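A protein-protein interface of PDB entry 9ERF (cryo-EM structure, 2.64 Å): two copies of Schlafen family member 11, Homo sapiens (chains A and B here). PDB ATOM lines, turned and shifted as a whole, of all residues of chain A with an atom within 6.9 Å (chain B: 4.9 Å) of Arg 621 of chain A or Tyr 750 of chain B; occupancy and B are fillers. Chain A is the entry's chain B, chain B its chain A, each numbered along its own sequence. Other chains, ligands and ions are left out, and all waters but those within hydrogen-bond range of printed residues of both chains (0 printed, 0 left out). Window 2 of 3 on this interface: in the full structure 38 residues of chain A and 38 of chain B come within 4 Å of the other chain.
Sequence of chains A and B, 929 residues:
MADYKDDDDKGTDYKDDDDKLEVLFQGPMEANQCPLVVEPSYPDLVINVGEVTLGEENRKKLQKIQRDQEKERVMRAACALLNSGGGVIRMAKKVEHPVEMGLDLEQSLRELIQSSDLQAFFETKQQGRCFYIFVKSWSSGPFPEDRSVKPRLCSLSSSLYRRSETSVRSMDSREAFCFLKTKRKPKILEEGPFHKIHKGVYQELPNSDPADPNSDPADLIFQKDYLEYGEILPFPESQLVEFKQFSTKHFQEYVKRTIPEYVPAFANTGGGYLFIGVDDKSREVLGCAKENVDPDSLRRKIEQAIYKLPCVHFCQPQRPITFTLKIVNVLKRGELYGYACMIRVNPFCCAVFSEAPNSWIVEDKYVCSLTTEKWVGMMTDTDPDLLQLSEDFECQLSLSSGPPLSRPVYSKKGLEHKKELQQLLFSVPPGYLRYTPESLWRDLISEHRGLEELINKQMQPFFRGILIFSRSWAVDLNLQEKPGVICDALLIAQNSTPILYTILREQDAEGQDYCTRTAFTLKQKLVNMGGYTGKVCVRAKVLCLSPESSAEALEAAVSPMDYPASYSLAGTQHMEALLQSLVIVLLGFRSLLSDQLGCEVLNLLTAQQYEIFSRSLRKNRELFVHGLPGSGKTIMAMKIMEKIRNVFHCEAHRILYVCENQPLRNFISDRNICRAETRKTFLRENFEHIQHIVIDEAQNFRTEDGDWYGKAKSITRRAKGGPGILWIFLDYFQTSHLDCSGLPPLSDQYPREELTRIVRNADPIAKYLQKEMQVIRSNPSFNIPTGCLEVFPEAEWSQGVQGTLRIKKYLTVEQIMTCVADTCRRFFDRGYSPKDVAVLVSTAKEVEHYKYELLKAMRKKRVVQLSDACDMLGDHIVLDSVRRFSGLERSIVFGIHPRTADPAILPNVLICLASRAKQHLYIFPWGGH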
ATOM      1  N   SER A 616      13.639 -12.783  10.212  1.00  0.00           N
ATOM      2  CA  SER A 616      14.073 -13.944   9.448  1.00  0.00           C
ATOM      3  C   SER A 616      14.225 -15.188  10.312  1.00  0.00           C
ATOM      4  O   SER A 616      14.402 -16.282   9.770  1.00  0.00           O
ATOM      5  CB  SER A 616      15.397 -13.639   8.751  1.00  0.00           C
ATOM      6  OG  SER A 616      15.370 -12.363   8.141  1.00  0.00           O
ATOM      7  N   LEU A 617      14.173 -15.050  11.638  1.00  0.00           N
ATOM      8  CA  LEU A 617      14.368 -16.211  12.502  1.00  0.00           C
ATOM      9  C   LEU A 617      13.247 -17.227  12.332  1.00  0.00           C
ATOM     10  O   LEU A 617      13.500 -18.434  12.257  1.00  0.00           O
ATOM     11  CB  LEU A 617      14.467 -15.766  13.959  1.00  0.00           C
ATOM     12  CG  LEU A 617      14.837 -16.865  14.958  1.00  0.00           C
ATOM     13  CD1 LEU A 617      16.214 -17.427  14.653  1.00  0.00           C
ATOM     14  CD2 LEU A 617      14.771 -16.338  16.378  1.00  0.00           C
ATOM     15  N   ARG A 618      11.999 -16.759  12.279  1.00  0.00           N
ATOM     16  CA  ARG A 618      10.875 -17.667  12.075  1.00  0.00           C
ATOM     17  C   ARG A 618      10.924 -18.310  10.698  1.00  0.00           C
ATOM     18  O   ARG A 618      10.531 -19.471  10.541  1.00  0.00           O
ATOM     19  CB  ARG A 618       9.559 -16.907  12.262  1.00  0.00           C
ATOM     20  CG  ARG A 618       8.296 -17.700  11.929  1.00  0.00           C
ATOM     21  CD  ARG A 618       7.119 -16.781  11.616  1.00  0.00           C
ATOM     22  NE  ARG A 618       6.216 -16.600  12.746  1.00  0.00           N
ATOM     23  CZ  ARG A 618       5.527 -17.573  13.327  1.00  0.00           C
ATOM     24  NH1 ARG A 618       5.600 -18.824  12.902  1.00  0.00           N
ATOM     25  NH2 ARG A 618       4.736 -17.282  14.355  1.00  0.00           N
ATOM     26  N   LYS A 619      11.408 -17.582   9.697  1.00  0.00           N
ATOM     27  CA  LYS A 619      11.312 -17.998   8.309  1.00  0.00           C
ATOM     28  C   LYS A 619      12.475 -18.858   7.841  1.00  0.00           C
ATOM     29  O   LYS A 619      12.401 -19.414   6.741  1.00  0.00           O
ATOM     30  CB  LYS A 619      11.219 -16.759   7.415  1.00  0.00           C
ATOM     31  CG  LYS A 619      10.188 -15.754   7.884  1.00  0.00           C
ATOM     32  CD  LYS A 619       9.730 -14.840   6.761  1.00  0.00           C
ATOM     33  CE  LYS A 619      10.642 -13.638   6.601  1.00  0.00           C
ATOM     34  NZ  LYS A 619       9.887 -12.361   6.740  1.00  0.00           N
ATOM     35  N   ASN A 620      13.537 -18.992   8.630  1.00  0.00           N
ATOM     36  CA  ASN A 620      14.734 -19.680   8.172  1.00  0.00           C
ATOM     37  C   ASN A 620      15.257 -20.609   9.254  1.00  0.00           C
ATOM     38  O   ASN A 620      15.130 -20.345  10.450  1.00  0.00           O
ATOM     39  CB  ASN A 620      15.838 -18.692   7.778  1.00  0.00           C
ATOM     40  CG  ASN A 620      15.425 -17.777   6.650  1.00  0.00           C
ATOM     41  OD1 ASN A 620      15.486 -18.150   5.482  1.00  0.00           O
ATOM     42  ND2 ASN A 620      15.007 -16.568   6.994  1.00  0.00           N
ATOM     43  N   ARG A 621      15.851 -21.715   8.802  1.00  0.00           N
ATOM     44  CA  ARG A 621      16.675 -22.563   9.657  1.00  0.00           C
ATOM     45  C   ARG A 621      18.133 -22.415   9.245  1.00  0.00           C
ATOM     46  O   ARG A 621      18.977 -22.110  10.088  1.00  0.00           O
ATOM     47  CB  ARG A 621      16.214 -24.020   9.578  1.00  0.00           C
ATOM     48  CG  ARG A 621      15.357 -24.498  10.750  1.00  0.00           C
ATOM     49  CD  ARG A 621      14.345 -23.456  11.204  1.00  0.00           C
ATOM     50  NE  ARG A 621      13.498 -23.950  12.280  1.00  0.00           N
ATOM     51  CZ  ARG A 621      12.766 -23.176  13.072  1.00  0.00           C
ATOM     52  NH1 ARG A 621      12.741 -21.862  12.924  1.00  0.00           N
ATOM     53  NH2 ARG A 621      12.036 -23.736  14.030  1.00  0.00           N
ATOM     54  N   GLU A 622      18.453 -22.618   7.971  1.00  0.00           N
ATOM     55  CA  GLU A 622      19.749 -22.230   7.441  1.00  0.00           C
ATOM     56  C   GLU A 622      19.648 -20.844   6.823  1.00  0.00           C
ATOM     57  O   GLU A 622      18.723 -20.556   6.063  1.00  0.00           O
ATOM     58  CB  GLU A 622      20.212 -23.226   6.385  1.00  0.00           C
ATOM     59  CG  GLU A 622      20.297 -24.658   6.865  1.00  0.00           C
ATOM     60  CD  GLU A 622      21.346 -25.455   6.119  1.00  0.00           C
ATOM     61  OE1 GLU A 622      21.078 -26.632   5.803  1.00  0.00           O
ATOM     62  OE2 GLU A 622      22.436 -24.908   5.854  1.00  0.00           O
ATOM     63  N   LEU A 623      20.598 -19.977   7.155  1.00  0.00           N
ATOM     64  CA  LEU A 623      20.607 -18.633   6.601  1.00  0.00           C
ATOM     65  C   LEU A 623      22.043 -18.159   6.455  1.00  0.00           C
ATOM     66  O   LEU A 623      22.827 -18.232   7.402  1.00  0.00           O
ATOM     67  CB  LEU A 623      19.811 -17.666   7.484  1.00  0.00           C
ATOM     68  CG  LEU A 623      19.650 -16.245   6.948  1.00  0.00           C
ATOM     69  CD1 LEU A 623      18.887 -16.252   5.638  1.00  0.00           C
ATOM     70  CD2 LEU A 623      18.950 -15.374   7.971  1.00  0.00           C
ATOM     71  N   PHE A 648      13.256 -20.411  21.314  1.00  0.00           N
ATOM     72  CA  PHE A 648      13.272 -21.862  21.417  1.00  0.00           C
ATOM     73  C   PHE A 648      13.297 -22.353  22.856  1.00  0.00           C
ATOM     74  O   PHE A 648      13.261 -23.568  23.078  1.00  0.00           O
ATOM     75  CB  PHE A 648      14.478 -22.438  20.666  1.00  0.00           C
ATOM     76  CG  PHE A 648      14.322 -22.435  19.171  1.00  0.00           C
ATOM     77  CD1 PHE A 648      13.957 -21.284  18.496  1.00  0.00           C
ATOM     78  CD2 PHE A 648      14.531 -23.593  18.442  1.00  0.00           C
ATOM     79  CE1 PHE A 648      13.812 -21.286  17.123  1.00  0.00           C
ATOM     80  CE2 PHE A 648      14.388 -23.601  17.069  1.00  0.00           C
ATOM     81  CZ  PHE A 648      14.026 -22.445  16.410  1.00  0.00           C
ATOM     82  N   ILE A 693      23.777 -23.336  15.972  1.00  0.00           N
ATOM     83  CA  ILE A 693      25.128 -22.859  15.703  1.00  0.00           C
ATOM     84  C   ILE A 693      25.037 -21.540  14.950  1.00  0.00           C
ATOM     85  O   ILE A 693      24.331 -21.444  13.940  1.00  0.00           O
ATOM     86  CB  ILE A 693      25.947 -23.885  14.902  1.00  0.00           C
ATOM     87  CG1 ILE A 693      26.082 -25.187  15.697  1.00  0.00           C
ATOM     88  CG2 ILE A 693      27.318 -23.318  14.564  1.00  0.00           C
ATOM     89  CD1 ILE A 693      26.864 -26.271  14.984  1.00  0.00           C
ATOM     90  N   GLY A 721      14.005 -29.582  17.829  1.00  0.00           N
ATOM     91  CA  GLY A 721      13.056 -28.807  17.055  1.00  0.00           C
ATOM     92  C   GLY A 721      13.291 -28.965  15.568  1.00  0.00           C
ATOM     93  O   GLY A 721      13.473 -27.975  14.853  1.00  0.00           O
ATOM     94  N   GLY A 722      13.294 -30.208  15.091  1.00  0.00           N
ATOM     95  CA  GLY A 722      13.648 -30.489  13.721  1.00  0.00           C
ATOM     96  C   GLY A 722      15.096 -30.124  13.475  1.00  0.00           C
ATOM     97  O   GLY A 722      15.930 -30.195  14.382  1.00  0.00           O
ATOM     98  N   PRO A 723      15.432 -29.721  12.251  1.00  0.00           N
ATOM     99  CA  PRO A 723      16.782 -29.194  12.015  1.00  0.00           C
ATOM    100  C   PRO A 723      16.981 -27.888  12.765  1.00  0.00           C
ATOM    101  O   PRO A 723      16.157 -26.974  12.687  1.00  0.00           O
ATOM    102  CB  PRO A 723      16.830 -28.998  10.495  1.00  0.00           C
ATOM    103  CG  PRO A 723      15.412 -28.871  10.075  1.00  0.00           C
ATOM    104  CD  PRO A 723      14.608 -29.704  11.030  1.00  0.00           C
ATOM    105  N   GLY A 724      18.085 -27.805  13.499  1.00  0.00           N
ATOM    106  CA  GLY A 724      18.366 -26.642  14.309  1.00  0.00           C
ATOM    107  C   GLY A 724      18.801 -25.454  13.474  1.00  0.00           C
ATOM    108  O   GLY A 724      19.025 -25.535  12.266  1.00  0.00           O
ATOM    109  N   ILE A 725      18.917 -24.313  14.152  1.00  0.00           N
ATOM    110  CA  ILE A 725      19.357 -23.088  13.497  1.00  0.00           C
ATOM    111  C   ILE A 725      20.821 -23.221  13.101  1.00  0.00           C
ATOM    112  O   ILE A 725      21.655 -23.687  13.885  1.00  0.00           O
ATOM    113  CB  ILE A 725      19.143 -21.879  14.420  1.00  0.00           C
ATOM    114  CG1 ILE A 725      17.650 -21.641  14.671  1.00  0.00           C
ATOM    115  CG2 ILE A 725      19.792 -20.642  13.836  1.00  0.00           C
ATOM    116  CD1 ILE A 725      16.872 -21.193  13.451  1.00  0.00           C
ATOM    117  N   LEU A 726      21.135 -22.820  11.871  1.00  0.00           N
ATOM    118  CA  LEU A 726      22.512 -22.717  11.389  1.00  0.00           C
ATOM    119  C   LEU A 726      22.610 -21.430  10.578  1.00  0.00           C
ATOM    120  O   LEU A 726      22.375 -21.431   9.368  1.00  0.00           O
ATOM    121  CB  LEU A 726      22.910 -23.933  10.562  1.00  0.00           C
ATOM    122  CG  LEU A 726      24.251 -23.815   9.834  1.00  0.00           C
ATOM    123  CD1 LEU A 726      25.366 -23.501  10.808  1.00  0.00           C
ATOM    124  CD2 LEU A 726      24.558 -25.088   9.076  1.00  0.00           C
ATOM    125  N   TRP A 727      22.967 -20.338  11.243  1.00  0.00           N
ATOM    126  CA  TRP A 727      23.131 -19.047  10.591  1.00  0.00           C
ATOM    127  C   TRP A 727      24.614 -18.731  10.472  1.00  0.00           C
ATOM    128  O   TRP A 727      25.357 -18.837  11.452  1.00  0.00           O
ATOM    129  CB  TRP A 727      22.405 -17.949  11.365  1.00  0.00           C
ATOM    130  CG  TRP A 727      20.929 -17.966  11.130  1.00  0.00           C
ATOM    131  CD1 TRP A 727      20.175 -19.036  10.754  1.00  0.00           C
ATOM    132  CD2 TRP A 727      20.027 -16.863  11.245  1.00  0.00           C
ATOM    133  NE1 TRP A 727      18.861 -18.673  10.631  1.00  0.00           N
ATOM    134  CE2 TRP A 727      18.742 -17.342  10.928  1.00  0.00           C
ATOM    135  CE3 TRP A 727      20.178 -15.518  11.587  1.00  0.00           C
ATOM    136  CZ2 TRP A 727      17.619 -16.526  10.942  1.00  0.00           C
ATOM    137  CZ3 TRP A 727      19.060 -14.711  11.599  1.00  0.00           C
ATOM    138  CH2 TRP A 727      17.799 -15.216  11.280  1.00  0.00           C
ATOM    139  N   PRO A 751      19.133 -19.884   1.783  1.00  0.00           N
ATOM    140  CA  PRO A 751      18.623 -18.518   1.586  1.00  0.00           C
ATOM    141  C   PRO A 751      19.597 -17.460   2.097  1.00  0.00           C
ATOM    142  O   PRO A 751      20.470 -17.763   2.900  1.00  0.00           O
ATOM    143  CB  PRO A 751      17.315 -18.524   2.384  1.00  0.00           C
ATOM    144  CG  PRO A 751      17.537 -19.532   3.459  1.00  0.00           C
ATOM    145  CD  PRO A 751      18.381 -20.599   2.828  1.00  0.00           C
ATOM    146  N   PHE B 624       8.925 -22.268   0.584  1.00  0.00           N
ATOM    147  CA  PHE B 624       7.605 -22.807   0.869  1.00  0.00           C
ATOM    148  C   PHE B 624       6.726 -21.664   1.351  1.00  0.00           C
ATOM    149  O   PHE B 624       7.030 -21.030   2.365  1.00  0.00           O
ATOM    150  CB  PHE B 624       7.677 -23.912   1.920  1.00  0.00           C
ATOM    151  CG  PHE B 624       8.363 -25.156   1.444  1.00  0.00           C
ATOM    152  CD1 PHE B 624       9.742 -25.256   1.473  1.00  0.00           C
ATOM    153  CD2 PHE B 624       7.629 -26.230   0.975  1.00  0.00           C
ATOM    154  CE1 PHE B 624      10.375 -26.399   1.039  1.00  0.00           C
ATOM    155  CE2 PHE B 624       8.259 -27.374   0.542  1.00  0.00           C
ATOM    156  CZ  PHE B 624       9.633 -27.459   0.573  1.00  0.00           C
ATOM    157  N   LEU B 746       6.855 -30.820   7.772  1.00  0.00           N
ATOM    158  CA  LEU B 746       6.782 -29.436   8.218  1.00  0.00           C
ATOM    159  C   LEU B 746       8.094 -28.962   8.824  1.00  0.00           C
ATOM    160  O   LEU B 746       8.349 -27.753   8.856  1.00  0.00           O
ATOM    161  CB  LEU B 746       5.650 -29.278   9.233  1.00  0.00           C
ATOM    162  CG  LEU B 746       5.351 -27.852   9.698  1.00  0.00           C
ATOM    163  CD1 LEU B 746       4.849 -27.003   8.542  1.00  0.00           C
ATOM    164  CD2 LEU B 746       4.345 -27.865  10.833  1.00  0.00           C
ATOM    165  N   SER B 747       8.927 -29.882   9.314  1.00  0.00           N
ATOM    166  CA  SER B 747      10.250 -29.507   9.793  1.00  0.00           C
ATOM    167  C   SER B 747      11.203 -29.201   8.649  1.00  0.00           C
ATOM    168  O   SER B 747      12.114 -28.385   8.820  1.00  0.00           O
ATOM    169  CB  SER B 747      10.834 -30.624  10.657  1.00  0.00           C
ATOM    170  OG  SER B 747      10.923 -31.835   9.927  1.00  0.00           O
ATOM    171  N   ASP B 748      11.018 -29.839   7.495  1.00  0.00           N
ATOM    172  CA  ASP B 748      11.882 -29.644   6.342  1.00  0.00           C
ATOM    173  C   ASP B 748      11.343 -28.621   5.352  1.00  0.00           C
ATOM    174  O   ASP B 748      12.006 -28.351   4.347  1.00  0.00           O
ATOM    175  CB  ASP B 748      12.098 -30.977   5.621  1.00  0.00           C
ATOM    176  CG  ASP B 748      12.786 -32.004   6.495  1.00  0.00           C
ATOM    177  OD1 ASP B 748      12.107 -32.602   7.357  1.00  0.00           O
ATOM    178  OD2 ASP B 748      14.004 -32.213   6.324  1.00  0.00           O
ATOM    179  N   GLN B 749      10.161 -28.059   5.599  1.00  0.00           N
ATOM    180  CA  GLN B 749       9.593 -27.044   4.708  1.00  0.00           C
ATOM    181  C   GLN B 749      10.176 -25.672   5.056  1.00  0.00           C
ATOM    182  O   GLN B 749       9.520 -24.795   5.622  1.00  0.00           O
ATOM    183  CB  GLN B 749       8.075 -27.050   4.796  1.00  0.00           C
ATOM    184  CG  GLN B 749       7.435 -28.241   4.108  1.00  0.00           C
ATOM    185  CD  GLN B 749       5.935 -28.278   4.277  1.00  0.00           C
ATOM    186  OE1 GLN B 749       5.292 -27.243   4.436  1.00  0.00           O
ATOM    187  NE2 GLN B 749       5.365 -29.473   4.235  1.00  0.00           N
ATOM    188  N   TYR B 750      11.445 -25.498   4.697  1.00  0.00           N
ATOM    189  CA  TYR B 750      12.179 -24.263   4.927  1.00  0.00           C
ATOM    190  C   TYR B 750      13.056 -23.965   3.721  1.00  0.00           C
ATOM    191  O   TYR B 750      13.512 -24.892   3.040  1.00  0.00           O
ATOM    192  CB  TYR B 750      13.053 -24.353   6.185  1.00  0.00           C
ATOM    193  CG  TYR B 750      12.285 -24.161   7.466  1.00  0.00           C
ATOM    194  CD1 TYR B 750      11.904 -22.896   7.883  1.00  0.00           C
ATOM    195  CD2 TYR B 750      11.930 -25.243   8.253  1.00  0.00           C
ATOM    196  CE1 TYR B 750      11.199 -22.715   9.048  1.00  0.00           C
ATOM    197  CE2 TYR B 750      11.224 -25.071   9.421  1.00  0.00           C
ATOM    198  CZ  TYR B 750      10.860 -23.806   9.814  1.00  0.00           C
ATOM    199  OH  TYR B 750      10.154 -23.629  10.980  1.00  0.00           O
ATOM    200  N   PRO B 751      13.308 -22.682   3.425  1.00  0.00           N
ATOM    201  CA  PRO B 751      12.804 -21.476   4.100  1.00  0.00           C
ATOM    202  C   PRO B 751      11.309 -21.292   3.872  1.00  0.00           C
ATOM    203  O   PRO B 751      10.741 -21.885   2.964  1.00  0.00           O
ATOM    204  CB  PRO B 751      13.636 -20.352   3.469  1.00  0.00           C
ATOM    205  CG  PRO B 751      14.004 -20.865   2.122  1.00  0.00           C
ATOM    206  CD  PRO B 751      14.201 -22.343   2.305  1.00  0.00           C
ATOM    207  N   ARG B 752      10.644 -20.479   4.685  1.00  0.00           N
ATOM    208  CA  ARG B 752       9.194 -20.391   4.681  1.00  0.00           C
ATOM    209  C   ARG B 752       8.753 -18.938   4.604  1.00  0.00           C
ATOM    210  O   ARG B 752       9.396 -18.051   5.168  1.00  0.00           O
ATOM    211  CB  ARG B 752       8.611 -21.038   5.934  1.00  0.00           C
ATOM    212  CG  ARG B 752       7.141 -21.369   5.835  1.00  0.00           C
ATOM    213  CD  ARG B 752       6.686 -22.184   7.025  1.00  0.00           C
ATOM    214  NE  ARG B 752       7.415 -23.440   7.138  1.00  0.00           N
ATOM    215  CZ  ARG B 752       7.394 -24.224   8.206  1.00  0.00           C
ATOM    216  NH1 ARG B 752       6.703 -23.900   9.287  1.00  0.00           N
ATOM    217  NH2 ARG B 752       8.082 -25.359   8.191  1.00  0.00           N
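Hydrophobic or aromatic side chains of chain A that line the printed part of chain B: Pro 723 and Pro 751. Among the printed residues, 8 pairs touch across the chains. Among the printed residues, no Asp or Glu carboxylate lies within 4 Å of a Lys or Arg side-chain nitrogen of the other chain.
N of Arg 752 of chain B sits at hydrogen-bond distance from O of Lys 619 of chain A (2.9 Å).
NH2 of Arg 752 of chain B lies within hydrogen-bond range of O of Leu 746 of chain B, 2.5 Å away. The side-chain hydroxyl (OG) of Ser 747 of chain B is in hydrogen-bond range of the side-chain carboxylate (OD1) of Asp 748 of chain B (2.9 Å). O of Arg 621 of chain A sits close to NE1 of Trp 727 of chain A (3.5 Å). The guanidinium group of Arg 752 of chain B is in hydrogen-bond range of the backbone carbonyl oxygen of Gln 749 of chain B (2.9 Å). ND2 of Asn 620 of chain A sits at hydrogen-bond distance from O of Ser 616 of chain A (2.9 Å). O of Arg 621 of chain A sits at hydrogen-bond distance from N of Leu 726 of chain A, at 2.9 Å.
Pro 751 of chain B touches its own counterpart, Pro 751 of chain A. Of the 8 pairs that touch across the chains among the printed residues, 1 has its exchanged pair printed and touching as well.
Of the printed residues of chain B, Lys 619 of chain A touches Tyr 750, Pro 751 and Arg 752. Of chain B, only Tyr 750 comes within 4 Å of Arg 621 of chain A. Phe 648 of chain A touches none of the printed residues of chain B. Gly 722 of chain A touches none of the printed residues of chain B. Printed residues of chain B within 4 Å of Pro 723 of chain A: Ser 747. Of the printed residues of chain A, Ser 747 of chain B touches Pro 723. Of chain A, only Arg 618, Lys 619 and Arg 621 come within 4 Å of Tyr 750 of chain B. Printed residues of chain A within 4 Å of Pro 751 of chain B: Lys 619, Asn 620 and Pro 751. The nearest printed residue of chain B that does not touch Arg 621 of chain A is Ser 747 of chain B (5.4 Å). The nearest residue of chain A that does not touch Tyr 750 of chain B is Asn 620 of chain A (4.3 Å). The nearest printed residue of chain B that does not touch Asn 620 of chain A is Tyr 750 of chain B (4.3 Å).
Tyr 750 of chain B touches Arg 618 of chain A. Lys 619 of chain A touches Tyr 750 of chain B. Lys 619 of chain A touches Pro 751 of chain B. Asn 620 of chain A touches Pro 751 of chain B. Arg 621 of chain A touches Tyr 750 of chain B (CZ to OH, 3.4 Å). Pro 723 of chain A touches Ser 747 of chain B (CG to O, 3.6 Å). Pro 751 of chain A touches Pro 751 of chain B (CG to CB, 3.99 Å).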
